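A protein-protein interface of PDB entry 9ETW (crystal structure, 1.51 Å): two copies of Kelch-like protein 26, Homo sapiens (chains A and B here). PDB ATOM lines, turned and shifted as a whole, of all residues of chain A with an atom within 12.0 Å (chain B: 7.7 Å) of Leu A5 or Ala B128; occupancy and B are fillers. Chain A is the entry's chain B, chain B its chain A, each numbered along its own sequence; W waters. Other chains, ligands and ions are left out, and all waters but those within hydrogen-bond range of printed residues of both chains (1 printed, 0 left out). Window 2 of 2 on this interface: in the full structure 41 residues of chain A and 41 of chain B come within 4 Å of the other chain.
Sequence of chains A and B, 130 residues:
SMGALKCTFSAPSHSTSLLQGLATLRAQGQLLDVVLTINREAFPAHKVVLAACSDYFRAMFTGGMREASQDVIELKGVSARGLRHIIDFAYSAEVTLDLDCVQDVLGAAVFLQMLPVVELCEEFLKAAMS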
ATOM      1  N   LEU A   5      29.512  -0.530 -18.462  1.00  0.00           N
ATOM      2  CA  LEU A   5      28.712  -1.222 -19.478  1.00  0.00           C
ATOM      3  C   LEU A   5      27.908  -0.224 -20.321  1.00  0.00           C
ATOM      4  O   LEU A   5      27.056  -0.618 -21.120  1.00  0.00           O
ATOM      5  CB  LEU A   5      27.782  -2.247 -18.808  1.00  0.00           C
ATOM      6  CG  LEU A   5      27.018  -3.217 -19.712  1.00  0.00           C
ATOM      7  CD1 LEU A   5      27.929  -3.833 -20.762  1.00  0.00           C
ATOM      8  CD2 LEU A   5      26.371  -4.314 -18.870  1.00  0.00           C
ATOM      9  N   LYS A   6      28.210   1.063 -20.148  1.00  0.00           N
ATOM     10  CA  LYS A   6      27.445   2.126 -20.785  1.00  0.00           C
ATOM     11  C   LYS A   6      27.395   1.961 -22.299  1.00  0.00           C
ATOM     12  O   LYS A   6      28.427   1.795 -22.957  1.00  0.00           O
ATOM     13  CB  LYS A   6      28.051   3.484 -20.433  1.00  0.00           C
ATOM     14  CG  LYS A   6      27.126   4.654 -20.697  1.00  0.00           C
ATOM     15  CD  LYS A   6      27.577   5.877 -19.911  1.00  0.00           C
ATOM     16  CE  LYS A   6      28.705   6.595 -20.622  1.00  0.00           C
ATOM     17  NZ  LYS A   6      29.710   7.163 -19.664  1.00  0.00           N
ATOM     18  N   CYS A   7      26.191   2.042 -22.853  1.00  0.00           N
ATOM     19  CA  CYS A   7      25.991   1.813 -24.272  1.00  0.00           C
ATOM     20  C   CYS A   7      24.891   2.728 -24.784  1.00  0.00           C
ATOM     21  O   CYS A   7      23.907   2.986 -24.084  1.00  0.00           O
ATOM     22  CB  CYS A   7      25.632   0.342 -24.544  1.00  0.00           C
ATOM     23  SG  CYS A   7      25.511  -0.060 -26.313  1.00  0.00           S
ATOM     24  N   THR A   8      25.052   3.203 -26.020  1.00  0.00           N
ATOM     25  CA  THR A   8      24.039   4.024 -26.673  1.00  0.00           C
ATOM     26  C   THR A   8      23.268   3.182 -27.685  1.00  0.00           C
ATOM     27  O   THR A   8      23.869   2.522 -28.534  1.00  0.00           O
ATOM     28  CB  THR A   8      24.686   5.230 -27.355  1.00  0.00           C
ATOM     29  OG1 THR A   8      25.303   6.043 -26.350  1.00  0.00           O
ATOM     30  CG2 THR A   8      23.651   6.064 -28.150  1.00  0.00           C
ATOM     31  N   PHE A   9      21.942   3.194 -27.576  1.00  0.00           N
ATOM     32  CA  PHE A   9      21.037   2.459 -28.454  1.00  0.00           C
ATOM     33  C   PHE A   9      20.230   3.448 -29.274  1.00  0.00           C
ATOM     34  O   PHE A   9      19.844   4.509 -28.773  1.00  0.00           O
ATOM     35  CB  PHE A   9      20.065   1.587 -27.662  1.00  0.00           C
ATOM     36  CG  PHE A   9      20.729   0.526 -26.851  1.00  0.00           C
ATOM     37  CD1 PHE A   9      21.254   0.816 -25.604  1.00  0.00           C
ATOM     38  CD2 PHE A   9      20.828  -0.765 -27.331  1.00  0.00           C
ATOM     39  CE1 PHE A   9      21.865  -0.158 -24.857  1.00  0.00           C
ATOM     40  CE2 PHE A   9      21.442  -1.746 -26.600  1.00  0.00           C
ATOM     41  CZ  PHE A   9      21.970  -1.451 -25.351  1.00  0.00           C
ATOM     42  N   LEU B  97      22.495   4.116 -21.920  1.00  0.00           N
ATOM     43  CA  LEU B  97      22.111   3.393 -20.711  1.00  0.00           C
ATOM     44  C   LEU B  97      23.320   2.787 -20.022  1.00  0.00           C
ATOM     45  O   LEU B  97      24.316   2.438 -20.658  1.00  0.00           O
ATOM     46  CB  LEU B  97      21.135   2.261 -21.021  1.00  0.00           C
ATOM     47  CG  LEU B  97      19.812   2.737 -21.632  1.00  0.00           C
ATOM     48  CD1 LEU B  97      19.039   1.530 -22.178  1.00  0.00           C
ATOM     49  CD2 LEU B  97      18.995   3.478 -20.587  1.00  0.00           C
ATOM     50  N   ASP B  98      23.206   2.667 -18.706  1.00  0.00           N
ATOM     51  CA  ASP B  98      24.117   1.844 -17.916  1.00  0.00           C
ATOM     52  C   ASP B  98      23.343   1.266 -16.749  1.00  0.00           C
ATOM     53  O   ASP B  98      22.155   1.566 -16.543  1.00  0.00           O
ATOM     54  CB  ASP B  98      25.355   2.635 -17.453  1.00  0.00           C
ATOM     55  CG  ASP B  98      25.003   3.882 -16.638  1.00  0.00           C
ATOM     56  OD1 ASP B  98      24.037   3.868 -15.848  1.00  0.00           O
ATOM     57  OD2 ASP B  98      25.728   4.892 -16.773  1.00  0.00           O
ATOM     58  N   LEU B  99      24.010   0.377 -15.998  1.00  0.00           N
ATOM     59  CA  LEU B  99      23.318  -0.310 -14.915  1.00  0.00           C
ATOM     60  C   LEU B  99      22.869   0.655 -13.830  1.00  0.00           C
ATOM     61  O   LEU B  99      21.917   0.356 -13.109  1.00  0.00           O
ATOM     62  CB  LEU B  99      24.202  -1.410 -14.319  1.00  0.00           C
ATOM     63  CG  LEU B  99      24.316  -2.641 -15.220  1.00  0.00           C
ATOM     64  CD1 LEU B  99      25.172  -3.715 -14.592  1.00  0.00           C
ATOM     65  CD2 LEU B  99      22.933  -3.162 -15.484  1.00  0.00           C
ATOM     66  N   VAL B 102      19.419   2.533 -15.570  1.00  0.00           N
ATOM     67  CA  VAL B 102      18.424   1.898 -16.438  1.00  0.00           C
ATOM     68  C   VAL B 102      17.084   1.708 -15.716  1.00  0.00           C
ATOM     69  O   VAL B 102      16.011   1.832 -16.326  1.00  0.00           O
ATOM     70  CB  VAL B 102      18.964   0.580 -17.018  1.00  0.00           C
ATOM     71  CG1 VAL B 102      19.312  -0.426 -15.912  1.00  0.00           C
ATOM     72  CG2 VAL B 102      17.943  -0.012 -18.021  1.00  0.00           C
ATOM     73  N   CYS B 121      15.503  -0.469 -23.250  1.00  0.00           N
ATOM     74  CA  CYS B 121      15.901  -0.823 -21.887  1.00  0.00           C
ATOM     75  C   CYS B 121      15.910  -2.335 -21.674  1.00  0.00           C
ATOM     76  O   CYS B 121      16.818  -2.881 -21.030  1.00  0.00           O
ATOM     77  CB  CYS B 121      14.961  -0.166 -20.879  1.00  0.00           C
ATOM     78  SG  CYS B 121      15.235   1.624 -20.659  1.00  0.00           S
ATOM     79  N   GLU B 122      14.893  -3.028 -22.189  1.00  0.00           N
ATOM     80  CA  GLU B 122      14.848  -4.481 -22.084  1.00  0.00           C
ATOM     81  C   GLU B 122      16.006  -5.125 -22.834  1.00  0.00           C
ATOM     82  O   GLU B 122      16.585  -6.116 -22.370  1.00  0.00           O
ATOM     83  CB  GLU B 122      13.499  -4.986 -22.599  1.00  0.00           C
ATOM     84  CG  GLU B 122      12.365  -4.596 -21.652  1.00  0.00           C
ATOM     85  CD  GLU B 122      10.963  -4.788 -22.229  1.00  0.00           C
ATOM     86  OE1 GLU B 122      10.796  -4.782 -23.480  1.00  0.00           O
ATOM     87  OE2 GLU B 122      10.016  -4.918 -21.412  1.00  0.00           O
ATOM     88  N   GLU B 123      16.346  -4.586 -24.003  1.00  0.00           N
ATOM     89  CA  GLU B 123      17.481  -5.112 -24.744  1.00  0.00           C
ATOM     90  C   GLU B 123      18.789  -4.909 -23.973  1.00  0.00           C
ATOM     91  O   GLU B 123      19.633  -5.813 -23.912  1.00  0.00           O
ATOM     92  CB  GLU B 123      17.527  -4.453 -26.124  1.00  0.00           C
ATOM     93  CG  GLU B 123      18.718  -4.859 -26.947  1.00  0.00           C
ATOM     94  CD  GLU B 123      18.717  -4.182 -28.321  1.00  0.00           C
ATOM     95  OE1 GLU B 123      17.679  -3.596 -28.700  1.00  0.00           O
ATOM     96  OE2 GLU B 123      19.757  -4.227 -29.011  1.00  0.00           O
ATOM     97  N   PHE B 124      18.970  -3.733 -23.373  1.00  0.00           N
ATOM     98  CA  PHE B 124      20.180  -3.509 -22.596  1.00  0.00           C
ATOM     99  C   PHE B 124      20.251  -4.483 -21.424  1.00  0.00           C
ATOM    100  O   PHE B 124      21.314  -5.046 -21.123  1.00  0.00           O
ATOM    101  CB  PHE B 124      20.221  -2.045 -22.130  1.00  0.00           C
ATOM    102  CG  PHE B 124      21.330  -1.763 -21.152  1.00  0.00           C
ATOM    103  CD1 PHE B 124      22.638  -1.626 -21.588  1.00  0.00           C
ATOM    104  CD2 PHE B 124      21.074  -1.700 -19.790  1.00  0.00           C
ATOM    105  CE1 PHE B 124      23.673  -1.396 -20.674  1.00  0.00           C
ATOM    106  CE2 PHE B 124      22.107  -1.473 -18.872  1.00  0.00           C
ATOM    107  CZ  PHE B 124      23.408  -1.320 -19.320  1.00  0.00           C
ATOM    108  N   LEU B 125      19.115  -4.705 -20.750  1.00  0.00           N
ATOM    109  CA  LEU B 125      19.136  -5.525 -19.540  1.00  0.00           C
ATOM    110  C   LEU B 125      19.368  -6.987 -19.886  1.00  0.00           C
ATOM    111  O   LEU B 125      20.089  -7.701 -19.179  1.00  0.00           O
ATOM    112  CB  LEU B 125      17.825  -5.358 -18.783  1.00  0.00           C
ATOM    113  CG  LEU B 125      17.658  -4.063 -17.992  1.00  0.00           C
ATOM    114  CD1 LEU B 125      16.213  -3.952 -17.600  1.00  0.00           C
ATOM    115  CD2 LEU B 125      18.551  -4.093 -16.758  1.00  0.00           C
ATOM    116  N   LYS B 126      18.811  -7.426 -21.012  1.00  0.00           N
ATOM    117  CA  LYS B 126      19.070  -8.778 -21.478  1.00  0.00           C
ATOM    118  C   LYS B 126      20.535  -8.952 -21.835  1.00  0.00           C
ATOM    119  O   LYS B 126      21.137  -9.994 -21.546  1.00  0.00           O
ATOM    120  CB  LYS B 126      18.162  -9.089 -22.669  1.00  0.00           C
ATOM    121  CG  LYS B 126      18.486 -10.404 -23.369  1.00  0.00           C
ATOM    122  CD  LYS B 126      17.910 -10.424 -24.806  1.00  0.00           C
ATOM    123  CE  LYS B 126      18.086  -9.055 -25.543  1.00  0.00           C
ATOM    124  NZ  LYS B 126      19.486  -8.414 -25.530  1.00  0.00           N
ATOM    125  N   ALA B 127      21.141  -7.932 -22.441  1.00  0.00           N
ATOM    126  CA  ALA B 127      22.558  -8.038 -22.771  1.00  0.00           C
ATOM    127  C   ALA B 127      23.430  -8.014 -21.517  1.00  0.00           C
ATOM    128  O   ALA B 127      24.416  -8.754 -21.430  1.00  0.00           O
ATOM    129  CB  ALA B 127      22.959  -6.923 -23.734  1.00  0.00           C
ATOM    130  N   ALA B 128      23.084  -7.177 -20.537  1.00  0.00           N
ATOM    131  CA  ALA B 128      23.913  -7.030 -19.341  1.00  0.00           C
ATOM    132  C   ALA B 128      23.975  -8.308 -18.531  1.00  0.00           C
ATOM    133  O   ALA B 128      24.976  -8.566 -17.860  1.00  0.00           O
ATOM    134  CB  ALA B 128      23.376  -5.901 -18.460  1.00  0.00           C
ATOM    135  N   MET B 129      22.901  -9.080 -18.525  1.00  0.00           N
ATOM    136  CA  MET B 129      22.900 -10.338 -17.795  1.00  0.00           C
ATOM    137  C   MET B 129      23.359 -11.464 -18.720  1.00  0.00           C
ATOM    138  O   MET B 129      23.857 -12.490 -18.261  1.00  0.00           O
ATOM    139  CB  MET B 129      21.512 -10.623 -17.220  1.00  0.00           C
ATOM    140  CG  MET B 129      20.932  -9.469 -16.380  1.00  0.00           C
ATOM    141  SD  MET B 129      21.751  -9.064 -14.801  1.00  0.00           S
ATOM    142  CE  MET B 129      22.957  -7.820 -15.253  1.00  0.00           C
HETATM  143  O   HOH W   1      26.897  -0.166 -16.980  1.00  0.00           O
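The backbone carbonyl oxygen of Cys A7 is in hydrogen-bond range of the backbone NH of Leu B97 (2.8 Å).
The backbone carbonyl oxygen (O) of Glu B123 is in hydrogen-bond range of the side-chain amino group (NZ) of Lys B126 (3.1 Å).
Among the printed residues, merely in contact across the chains: Leu A5 with Phe B124, Leu A5 with Ala B128, Lys A6 with Leu B97, Lys A6 with Asp B98, Phe A9 with Glu B123 and Phe A9 with Phe B124.
Printed residues of chain B within 4 Å of Leu A5: Phe B124 (3.5 Å) and Ala B128 (3.4 Å).
Of the printed residues of chain B, Lys A6 touches Leu B97 and Asp B98.
Of the printed residues of chain B, Cys A7 touches Leu B97 (2.8 Å).
Of the printed residues of chain B, Phe A9 touches Glu B123 (3.8 Å) and Phe B124 (3.7 Å).
Of the printed residues of chain A, Leu B97 touches Lys A6 and Cys A7.
Of the printed residues of chain A, Asp B98 touches Lys A6 (3.8 Å).
Leu B99 touches none of the printed residues of chain A.
Of the printed residues of chain A, Glu B123 touches Phe A9 (3.8 Å).
Phe B124 touches just these residues of chain A: Leu A5 and Phe A9.
No residue of chain A comes within 4 Å of Leu B125.
No residue of chain A comes within 4 Å of Lys B126.
No residue of chain A comes within 4 Å of Ala B127.
Ala B128 touches just one residue of chain A: Leu A5 (3.4 Å).
Met B129 touches none of the printed residues of chain A.
The nearest residue of chain B that does not touch Leu A5 is Leu B97 (4.1 Å).
The nearest printed residue of chain B that does not touch Phe A9 is Leu B97 (4.1 Å).
Along chain B the printed residues that touch a printed residue of chain A span positions 97 to 128.
Hydrophobic or aromatic side chains of chain A that line the printed part of chain B: Leu A5 and Phe A9.
Among the printed residues, 7 pairs touch across the chains.
Among the printed residues, no Asp or Glu carboxylate lies within 4 Å of a Lys or Arg side-chain nitrogen of the other chain.
No position is printed for both chains.
Water W1 lies within hydrogen-bond range of the backbone NH of Leu A5 (3.0 Å) and the backbone NH of Leu B99 (3.1 Å).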
